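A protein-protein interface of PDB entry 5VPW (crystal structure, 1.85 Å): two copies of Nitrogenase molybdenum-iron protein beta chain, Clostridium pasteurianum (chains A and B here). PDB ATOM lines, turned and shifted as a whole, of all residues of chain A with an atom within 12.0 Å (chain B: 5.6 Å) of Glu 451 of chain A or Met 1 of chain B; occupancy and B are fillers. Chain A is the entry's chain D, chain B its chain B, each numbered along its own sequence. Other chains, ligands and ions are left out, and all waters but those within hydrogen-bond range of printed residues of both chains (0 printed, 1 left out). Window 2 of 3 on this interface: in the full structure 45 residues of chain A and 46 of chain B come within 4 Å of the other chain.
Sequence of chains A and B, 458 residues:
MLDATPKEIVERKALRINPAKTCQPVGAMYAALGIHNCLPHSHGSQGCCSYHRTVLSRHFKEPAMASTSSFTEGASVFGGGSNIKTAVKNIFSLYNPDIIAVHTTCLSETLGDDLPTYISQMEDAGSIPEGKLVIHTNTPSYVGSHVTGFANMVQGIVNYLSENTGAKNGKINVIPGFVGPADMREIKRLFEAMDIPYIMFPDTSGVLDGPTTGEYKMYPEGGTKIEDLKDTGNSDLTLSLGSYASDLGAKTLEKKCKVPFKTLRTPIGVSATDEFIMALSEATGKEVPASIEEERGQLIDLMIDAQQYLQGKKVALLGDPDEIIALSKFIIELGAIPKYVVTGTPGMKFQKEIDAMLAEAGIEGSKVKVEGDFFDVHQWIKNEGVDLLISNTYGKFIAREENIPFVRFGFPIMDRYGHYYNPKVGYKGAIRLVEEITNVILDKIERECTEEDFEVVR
The side-chain carboxylate of Glu 451 of chain A is in hydrogen-bond range of the backbone NH of Met 1 of chain B (2.7 Å). NZ of Lys 396 of chain B is in salt-bridge range of OE2 of Glu 446 of chain A. The side-chain amino group (NZ) of Lys 396 of chain B is in hydrogen-bond range of the backbone carbonyl oxygen (O) of Glu 455 of chain A, 2.5 Å away. The guanidinium group (NH1) of Arg 400 of chain B lies within hydrogen-bond range of the backbone carbonyl oxygen (O) of Glu 446 of chain A (2.6 Å). The guanidinium group (NH1) of Arg 400 of chain B sits at hydrogen-bond distance from the backbone carbonyl oxygen (O) of Arg 447 of chain A. The backbone carbonyl oxygen (O) of Cys 449 of chain A lies within hydrogen-bond range of the guanidinium group (NH2) of Arg 400 of chain B (2.7 Å).
The backbone NH (N) of Met 1 of chain B lies within hydrogen-bond range of the side-chain carboxylate (OD1) of Asp 3 of chain B. SD of Met 1 of chain B lies close to NE of Arg 400 of chain B (3.7 Å). The side-chain sulfur (SG) of Cys 449 of chain A lies within hydrogen-bond range of the backbone carbonyl oxygen (O) of Glu 446 of chain A (3.8 Å). The side-chain carboxylate of Glu 446 of chain A lies within salt-bridge range of the guanidinium group of Arg 458 of chain A, at 3.1 Å. NH2 of Arg 447 of chain A lies within salt-bridge range of OE2 of Glu 448 of chain A. The backbone carbonyl oxygen (O) of Asp 453 of chain A lies within hydrogen-bond range of the side-chain sulfur (SG) of Cys 449 of chain A, 3.8 Å away.
NH2 of Arg 400 of chain B touches C of Thr 450 of chain A, at 3.8 Å. Arg 400 of chain B touches Glu 451 of chain A. Phe 454 of chain A touches Met 1 of chain B (CG to CE, 3.3 Å). Lys 396 of chain B touches Phe 454 of chain A (CG to CE2, 3.9 Å). Phe 397 of chain B touches Phe 454 of chain A (CE1 to CD2, 3.6 Å). Phe 454 of chain A touches Arg 400 of chain B. Val 456 of chain A touches Phe 397 of chain B (CG2 to CZ, 3.6 Å).
Glu 451 of chain A touches just these residues of chain B: Met 1 (2.7 Å) and Arg 400 (3.6 Å). Met 1 of chain B touches just these residues of chain A: Glu 451 and Phe 454. No residue of chain A comes within 4 Å of Asp 3 of chain B. Of chain A, only Glu 446, Arg 447, Cys 449, Thr 450, Glu 451 and Phe 454 come within 4 Å of Arg 400 of chain B. No residue of chain A comes within 4 Å of Glu 401 of chain B. Printed residues of chain B within 4 Å of Thr 450 of chain A: Arg 400. Printed residues of chain B within 4 Å of Glu 455 of chain A: Lys 396 (2.5 Å). Printed residues of chain B within 4 Å of Val 456 of chain A: Phe 397. Of the printed residues of chain B, Phe 454 of chain A touches Met 1, Lys 396, Phe 397 and Arg 400. Of the printed residues of chain A, Lys 396 of chain B touches Glu 446 (2.8 Å), Phe 454 (3.9 Å) and Glu 455 (2.5 Å). Asp 443 of chain A touches none of the printed residues of chain B. The nearest residue of chain B that does not touch Glu 451 of chain A is Glu 401 of chain B (4.9 Å). The nearest printed residue of chain B that does not touch Thr 450 of chain A is Met 1 of chain B (5.6 Å).
Of the 8 printed residues of chain B, 4 touch a printed residue of chain A. Of the 16 printed residues of chain A, 8 touch a printed residue of chain B. Among the printed residues, 13 pairs touch across the chains. Among the printed residues, Asp or Glu carboxylates within 4 Å of a Lys or Arg side-chain nitrogen of the other chain: Glu 446 of chain A with Lys 396 of chain B.
No position is printed for both chains. Of the 13 pairs that touch across the chains among the printed residues, none has its exchanged pair printed and touching as well.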
ATOM      1  N   ASP A 443     -27.784  33.572   2.706  1.00  0.00           N
ATOM      2  CA  ASP A 443     -26.334  33.488   2.459  1.00  0.00           C
ATOM      3  C   ASP A 443     -25.582  32.949   3.686  1.00  0.00           C
ATOM      4  O   ASP A 443     -24.630  32.203   3.541  1.00  0.00           O
ATOM      5  CB  ASP A 443     -25.736  34.872   2.133  1.00  0.00           C
ATOM      6  CG  ASP A 443     -26.003  35.343   0.707  1.00  0.00           C
ATOM      7  OD1 ASP A 443     -26.313  34.536  -0.181  1.00  0.00           O
ATOM      8  OD2 ASP A 443     -25.790  36.545   0.462  1.00  0.00           O
ATOM      9  N   LYS A 444     -25.988  33.359   4.883  1.00  0.00           N
ATOM     10  CA  LYS A 444     -25.339  32.910   6.095  1.00  0.00           C
ATOM     11  C   LYS A 444     -25.612  31.421   6.331  1.00  0.00           C
ATOM     12  O   LYS A 444     -24.676  30.654   6.563  1.00  0.00           O
ATOM     13  CB  LYS A 444     -25.754  33.709   7.340  1.00  0.00           C
ATOM     14  CG  LYS A 444     -25.042  33.154   8.576  1.00  0.00           C
ATOM     15  CD  LYS A 444     -25.264  33.947   9.840  1.00  0.00           C
ATOM     16  CE  LYS A 444     -24.682  33.168  11.010  1.00  0.00           C
ATOM     17  NZ  LYS A 444     -24.820  33.901  12.259  1.00  0.00           N
ATOM     18  N   ILE A 445     -26.872  31.020   6.238  1.00  0.00           N
ATOM     19  CA  ILE A 445     -27.220  29.599   6.377  1.00  0.00           C
ATOM     20  C   ILE A 445     -26.341  28.714   5.468  1.00  0.00           C
ATOM     21  O   ILE A 445     -25.825  27.666   5.908  1.00  0.00           O
ATOM     22  CB  ILE A 445     -28.708  29.367   6.050  1.00  0.00           C
ATOM     23  CG1 ILE A 445     -29.601  29.958   7.150  1.00  0.00           C
ATOM     24  CG2 ILE A 445     -28.967  27.879   5.861  1.00  0.00           C
ATOM     25  CD1 ILE A 445     -31.066  30.011   6.776  1.00  0.00           C
ATOM     26  N   GLU A 446     -26.183  29.125   4.204  1.00  0.00           N
ATOM     27  CA  GLU A 446     -25.470  28.323   3.208  1.00  0.00           C
ATOM     28  C   GLU A 446     -23.979  28.329   3.398  1.00  0.00           C
ATOM     29  O   GLU A 446     -23.297  27.386   3.005  1.00  0.00           O
ATOM     30  CB  GLU A 446     -25.817  28.750   1.773  1.00  0.00           C
ATOM     31  CG  GLU A 446     -27.328  28.711   1.538  1.00  0.00           C
ATOM     32  CD  GLU A 446     -27.734  28.780   0.078  1.00  0.00           C
ATOM     33  OE1 GLU A 446     -27.001  29.418  -0.710  1.00  0.00           O
ATOM     34  OE2 GLU A 446     -28.766  28.191  -0.250  1.00  0.00           O
ATOM     35  N   ARG A 447     -23.479  29.404   3.988  1.00  0.00           N
ATOM     36  CA  ARG A 447     -22.065  29.589   4.203  1.00  0.00           C
ATOM     37  C   ARG A 447     -21.611  28.711   5.353  1.00  0.00           C
ATOM     38  O   ARG A 447     -20.469  28.238   5.383  1.00  0.00           O
ATOM     39  CB  ARG A 447     -21.787  31.069   4.498  1.00  0.00           C
ATOM     40  CG  ARG A 447     -20.343  31.387   4.804  1.00  0.00           C
ATOM     41  CD  ARG A 447     -19.965  32.810   4.407  1.00  0.00           C
ATOM     42  NE  ARG A 447     -21.058  33.781   4.470  1.00  0.00           N
ATOM     43  CZ  ARG A 447     -21.599  34.267   5.588  1.00  0.00           C
ATOM     44  NH1 ARG A 447     -22.577  35.168   5.512  1.00  0.00           N
ATOM     45  NH2 ARG A 447     -21.184  33.854   6.780  1.00  0.00           N
ATOM     46  N   GLU A 448     -22.522  28.464   6.287  1.00  0.00           N
ATOM     47  CA  GLU A 448     -22.168  27.806   7.526  1.00  0.00           C
ATOM     48  C   GLU A 448     -22.712  26.402   7.702  1.00  0.00           C
ATOM     49  O   GLU A 448     -22.328  25.723   8.629  1.00  0.00           O
ATOM     50  CB  GLU A 448     -22.634  28.675   8.687  1.00  0.00           C
ATOM     51  CG  GLU A 448     -21.793  29.936   8.732  1.00  0.00           C
ATOM     52  CD  GLU A 448     -22.144  30.821   9.884  1.00  0.00           C
ATOM     53  OE1 GLU A 448     -22.893  30.364  10.776  1.00  0.00           O
ATOM     54  OE2 GLU A 448     -21.676  31.974   9.872  1.00  0.00           O
ATOM     55  N   CYS A 449     -23.606  25.958   6.834  1.00  0.00           N
ATOM     56  CA  CYS A 449     -24.120  24.631   6.984  1.00  0.00           C
ATOM     57  C   CYS A 449     -23.017  23.629   6.621  1.00  0.00           C
ATOM     58  O   CYS A 449     -22.077  23.920   5.879  1.00  0.00           O
ATOM     59  CB  CYS A 449     -25.416  24.422   6.172  1.00  0.00           C
ATOM     60  SG  CYS A 449     -25.241  24.479   4.384  1.00  0.00           S
ATOM     61  N   THR A 450     -23.102  22.446   7.198  1.00  0.00           N
ATOM     62  CA  THR A 450     -22.216  21.385   6.769  1.00  0.00           C
ATOM     63  C   THR A 450     -22.613  21.023   5.355  1.00  0.00           C
ATOM     64  O   THR A 450     -23.753  21.300   4.904  1.00  0.00           O
ATOM     65  CB  THR A 450     -22.350  20.142   7.654  1.00  0.00           C
ATOM     66  OG1 THR A 450     -23.736  19.749   7.718  1.00  0.00           O
ATOM     67  CG2 THR A 450     -21.833  20.446   9.062  1.00  0.00           C
ATOM     68  N   GLU A 451     -21.683  20.382   4.668  1.00  0.00           N
ATOM     69  CA  GLU A 451     -21.909  19.894   3.302  1.00  0.00           C
ATOM     70  C   GLU A 451     -23.151  18.999   3.104  1.00  0.00           C
ATOM     71  O   GLU A 451     -23.874  19.148   2.121  1.00  0.00           O
ATOM     72  CB  GLU A 451     -20.639  19.203   2.843  1.00  0.00           C
ATOM     73  CG  GLU A 451     -19.535  20.242   2.750  1.00  0.00           C
ATOM     74  CD  GLU A 451     -18.159  19.654   2.879  1.00  0.00           C
ATOM     75  OE1 GLU A 451     -17.912  18.875   3.829  1.00  0.00           O
ATOM     76  OE2 GLU A 451     -17.323  20.002   2.030  1.00  0.00           O
ATOM     77  N   GLU A 452     -23.405  18.101   4.057  1.00  0.00           N
ATOM     78  CA  GLU A 452     -24.585  17.206   4.010  1.00  0.00           C
ATOM     79  C   GLU A 452     -25.936  17.906   4.293  1.00  0.00           C
ATOM     80  O   GLU A 452     -26.996  17.313   4.113  1.00  0.00           O
ATOM     81  CB  GLU A 452     -24.420  16.031   4.989  1.00  0.00           C
ATOM     82  CG  GLU A 452     -24.656  16.383   6.457  1.00  0.00           C
ATOM     83  CD  GLU A 452     -23.371  16.569   7.250  1.00  0.00           C
ATOM     84  OE1 GLU A 452     -22.335  16.991   6.661  1.00  0.00           O
ATOM     85  OE2 GLU A 452     -23.411  16.287   8.471  1.00  0.00           O
ATOM     86  N   ASP A 453     -25.888  19.151   4.763  1.00  0.00           N
ATOM     87  CA  ASP A 453     -27.085  19.938   4.953  1.00  0.00           C
ATOM     88  C   ASP A 453     -27.207  20.950   3.825  1.00  0.00           C
ATOM     89  O   ASP A 453     -27.975  21.928   3.945  1.00  0.00           O
ATOM     90  CB  ASP A 453     -27.051  20.659   6.311  1.00  0.00           C
ATOM     91  CG  ASP A 453     -27.359  19.731   7.487  1.00  0.00           C
ATOM     92  OD1 ASP A 453     -27.560  18.502   7.284  1.00  0.00           O
ATOM     93  OD2 ASP A 453     -27.390  20.250   8.626  1.00  0.00           O
ATOM     94  N   PHE A 454     -26.466  20.710   2.733  1.00  0.00           N
ATOM     95  CA  PHE A 454     -26.469  21.595   1.553  1.00  0.00           C
ATOM     96  C   PHE A 454     -27.690  21.374   0.601  1.00  0.00           C
ATOM     97  O   PHE A 454     -28.185  20.276   0.449  1.00  0.00           O
ATOM     98  CB  PHE A 454     -25.140  21.480   0.822  1.00  0.00           C
ATOM     99  CG  PHE A 454     -24.683  22.773   0.211  1.00  0.00           C
ATOM    100  CD1 PHE A 454     -24.373  23.872   1.027  1.00  0.00           C
ATOM    101  CD2 PHE A 454     -24.563  22.903  -1.175  1.00  0.00           C
ATOM    102  CE1 PHE A 454     -23.957  25.077   0.477  1.00  0.00           C
ATOM    103  CE2 PHE A 454     -24.141  24.102  -1.731  1.00  0.00           C
ATOM    104  CZ  PHE A 454     -23.842  25.193  -0.904  1.00  0.00           C
ATOM    105  N   GLU A 455     -28.210  22.438   0.006  1.00  0.00           N
ATOM    106  CA  GLU A 455     -29.580  22.419  -0.510  1.00  0.00           C
ATOM    107  C   GLU A 455     -29.690  23.105  -1.819  1.00  0.00           C
ATOM    108  O   GLU A 455     -29.211  24.223  -1.944  1.00  0.00           O
ATOM    109  CB  GLU A 455     -30.519  23.221   0.405  1.00  0.00           C
ATOM    110  CG  GLU A 455     -30.619  22.782   1.850  1.00  0.00           C
ATOM    111  CD  GLU A 455     -31.314  21.447   2.033  1.00  0.00           C
ATOM    112  OE1 GLU A 455     -32.081  21.008   1.165  1.00  0.00           O
ATOM    113  OE2 GLU A 455     -31.059  20.816   3.061  1.00  0.00           O
ATOM    114  N   VAL A 456     -30.406  22.497  -2.763  1.00  0.00           N
ATOM    115  CA  VAL A 456     -30.619  23.145  -4.034  1.00  0.00           C
ATOM    116  C   VAL A 456     -31.808  24.107  -3.994  1.00  0.00           C
ATOM    117  O   VAL A 456     -31.715  25.193  -4.513  1.00  0.00           O
ATOM    118  CB  VAL A 456     -30.756  22.103  -5.163  1.00  0.00           C
ATOM    119  CG1 VAL A 456     -31.283  22.726  -6.419  1.00  0.00           C
ATOM    120  CG2 VAL A 456     -29.393  21.454  -5.428  1.00  0.00           C
ATOM    121  N   VAL A 457     -32.932  23.692  -3.411  1.00  0.00           N
ATOM    122  CA  VAL A 457     -34.121  24.552  -3.305  1.00  0.00           C
ATOM    123  C   VAL A 457     -34.171  25.121  -1.879  1.00  0.00           C
ATOM    124  O   VAL A 457     -33.756  24.447  -0.940  1.00  0.00           O
ATOM    125  CB  VAL A 457     -35.420  23.746  -3.559  1.00  0.00           C
ATOM    126  CG1 VAL A 457     -36.634  24.646  -3.663  1.00  0.00           C
ATOM    127  CG2 VAL A 457     -35.299  22.933  -4.840  1.00  0.00           C
ATOM    128  N   ARG A 458     -34.584  26.384  -1.769  1.00  0.00           N
ATOM    129  CA  ARG A 458     -34.882  27.039  -0.498  1.00  0.00           C
ATOM    130  C   ARG A 458     -36.176  27.792  -0.613  1.00  0.00           C
ATOM    131  O   ARG A 458     -36.653  28.063  -1.734  1.00  0.00           O
ATOM    132  CB  ARG A 458     -33.791  28.017  -0.074  1.00  0.00           C
ATOM    133  CG  ARG A 458     -32.411  27.412   0.054  1.00  0.00           C
ATOM    134  CD  ARG A 458     -32.095  27.091   1.466  1.00  0.00           C
ATOM    135  NE  ARG A 458     -30.699  26.705   1.637  1.00  0.00           N
ATOM    136  CZ  ARG A 458     -30.272  26.036   2.697  1.00  0.00           C
ATOM    137  NH1 ARG A 458     -31.133  25.696   3.650  1.00  0.00           N
ATOM    138  NH2 ARG A 458     -28.997  25.670   2.789  1.00  0.00           N
ATOM    139  OXT ARG A 458     -36.756  28.147   0.454  1.00  0.00           O
ATOM    140  N   MET B   1     -17.419  19.277  -0.536  1.00  0.00           N
ATOM    141  CA  MET B   1     -18.333  19.716  -1.621  1.00  0.00           C
ATOM    142  C   MET B   1     -17.697  19.421  -2.995  1.00  0.00           C
ATOM    143  O   MET B   1     -16.597  19.900  -3.309  1.00  0.00           O
ATOM    144  CB  MET B   1     -18.675  21.202  -1.444  1.00  0.00           C
ATOM    145  CG  MET B   1     -19.810  21.691  -2.340  1.00  0.00           C
ATOM    146  SD  MET B   1     -21.094  22.631  -1.475  1.00  0.00           S
ATOM    147  CE  MET B   1     -21.717  21.402  -0.322  1.00  0.00           C
ATOM    148  N   LEU B   2     -18.396  18.601  -3.786  1.00  0.00           N
ATOM    149  CA  LEU B   2     -17.906  18.087  -5.076  1.00  0.00           C
ATOM    150  C   LEU B   2     -16.484  17.485  -4.984  1.00  0.00           C
ATOM    151  O   LEU B   2     -15.573  17.881  -5.743  1.00  0.00           O
ATOM    152  CB  LEU B   2     -17.990  19.175  -6.154  1.00  0.00           C
ATOM    153  CG  LEU B   2     -19.375  19.807  -6.336  1.00  0.00           C
ATOM    154  CD1 LEU B   2     -19.314  20.815  -7.473  1.00  0.00           C
ATOM    155  CD2 LEU B   2     -20.453  18.765  -6.593  1.00  0.00           C
ATOM    156  N   ASP B   3     -16.329  16.521  -4.060  1.00  0.00           N
ATOM    157  CA  ASP B   3     -15.051  15.817  -3.784  1.00  0.00           C
ATOM    158  C   ASP B   3     -14.527  14.969  -4.953  1.00  0.00           C
ATOM    159  O   ASP B   3     -13.312  14.804  -5.110  1.00  0.00           O
ATOM    160  CB  ASP B   3     -15.189  14.880  -2.565  1.00  0.00           C
ATOM    161  CG  ASP B   3     -15.451  15.623  -1.272  1.00  0.00           C
ATOM    162  OD1 ASP B   3     -15.173  16.842  -1.208  1.00  0.00           O
ATOM    163  OD2 ASP B   3     -15.939  14.976  -0.315  1.00  0.00           O
ATOM    164  N   HIS B 378     -15.950  23.459 -13.637  1.00  0.00           N
ATOM    165  CA  HIS B 378     -15.370  23.244 -12.357  1.00  0.00           C
ATOM    166  C   HIS B 378     -13.939  22.772 -12.510  1.00  0.00           C
ATOM    167  O   HIS B 378     -13.040  23.241 -11.822  1.00  0.00           O
ATOM    168  CB  HIS B 378     -16.184  22.233 -11.539  1.00  0.00           C
ATOM    169  CG  HIS B 378     -15.774  22.171 -10.102  1.00  0.00           C
ATOM    170  ND1 HIS B 378     -16.271  21.233  -9.221  1.00  0.00           N
ATOM    171  CD2 HIS B 378     -14.890  22.919  -9.396  1.00  0.00           C
ATOM    172  CE1 HIS B 378     -15.728  21.421  -8.028  1.00  0.00           C
ATOM    173  NE2 HIS B 378     -14.875  22.428  -8.112  1.00  0.00           N
ATOM    174  N   LYS B 396     -23.969  27.106  -7.337  1.00  0.00           N
ATOM    175  CA  LYS B 396     -23.698  27.340  -5.949  1.00  0.00           C
ATOM    176  C   LYS B 396     -22.672  26.339  -5.415  1.00  0.00           C
ATOM    177  O   LYS B 396     -21.951  26.643  -4.478  1.00  0.00           O
ATOM    178  CB  LYS B 396     -25.014  27.301  -5.117  1.00  0.00           C
ATOM    179  CG  LYS B 396     -25.579  25.891  -4.868  1.00  0.00           C
ATOM    180  CD  LYS B 396     -27.009  25.929  -4.337  1.00  0.00           C
ATOM    181  CE  LYS B 396     -27.077  26.579  -2.993  1.00  0.00           C
ATOM    182  NZ  LYS B 396     -28.472  26.534  -2.514  1.00  0.00           N
ATOM    183  N   PHE B 397     -22.638  25.139  -5.975  1.00  0.00           N
ATOM    184  CA  PHE B 397     -21.709  24.128  -5.484  1.00  0.00           C
ATOM    185  C   PHE B 397     -20.265  24.550  -5.777  1.00  0.00           C
ATOM    186  O   PHE B 397     -19.397  24.505  -4.908  1.00  0.00           O
ATOM    187  CB  PHE B 397     -21.981  22.773  -6.146  1.00  0.00           C
ATOM    188  CG  PHE B 397     -23.349  22.205  -5.874  1.00  0.00           C
ATOM    189  CD1 PHE B 397     -23.732  21.861  -4.588  1.00  0.00           C
ATOM    190  CD2 PHE B 397     -24.230  21.958  -6.925  1.00  0.00           C
ATOM    191  CE1 PHE B 397     -24.973  21.301  -4.351  1.00  0.00           C
ATOM    192  CE2 PHE B 397     -25.469  21.397  -6.689  1.00  0.00           C
ATOM    193  CZ  PHE B 397     -25.843  21.079  -5.399  1.00  0.00           C
ATOM    194  N   ARG B 400     -19.229  27.598  -3.677  1.00  0.00           N
ATOM    195  CA  ARG B 400     -18.865  27.322  -2.297  1.00  0.00           C
ATOM    196  C   ARG B 400     -17.515  26.594  -2.237  1.00  0.00           C
ATOM    197  O   ARG B 400     -16.642  26.960  -1.451  1.00  0.00           O
ATOM    198  CB  ARG B 400     -19.981  26.546  -1.563  1.00  0.00           C
ATOM    199  CG  ARG B 400     -19.568  25.977  -0.205  1.00  0.00           C
ATOM    200  CD  ARG B 400     -20.791  25.576   0.639  1.00  0.00           C
ATOM    201  NE  ARG B 400     -20.457  24.566   1.658  1.00  0.00           N
ATOM    202  CZ  ARG B 400     -20.722  24.635   2.972  1.00  0.00           C
ATOM    203  NH1 ARG B 400     -21.354  25.669   3.503  1.00  0.00           N
ATOM    204  NH2 ARG B 400     -20.364  23.634   3.773  1.00  0.00           N
ATOM    205  N   GLU B 401     -17.356  25.578  -3.072  1.00  0.00           N
ATOM    206  CA  GLU B 401     -16.175  24.732  -3.050  1.00  0.00           C
ATOM    207  C   GLU B 401     -14.959  25.576  -3.423  1.00  0.00           C
ATOM    208  O   GLU B 401     -13.904  25.396  -2.846  1.00  0.00           O
ATOM    209  CB  GLU B 401     -16.372  23.495  -3.955  1.00  0.00           C
ATOM    210  CG  GLU B 401     -15.128  22.617  -4.222  1.00  0.00           C
ATOM    211  CD  GLU B 401     -14.497  21.943  -2.978  1.00  0.00           C
ATOM    212  OE1 GLU B 401     -15.068  21.998  -1.862  1.00  0.00           O
ATOM    213  OE2 GLU B 401     -13.418  21.324  -3.125  1.00  0.00           O
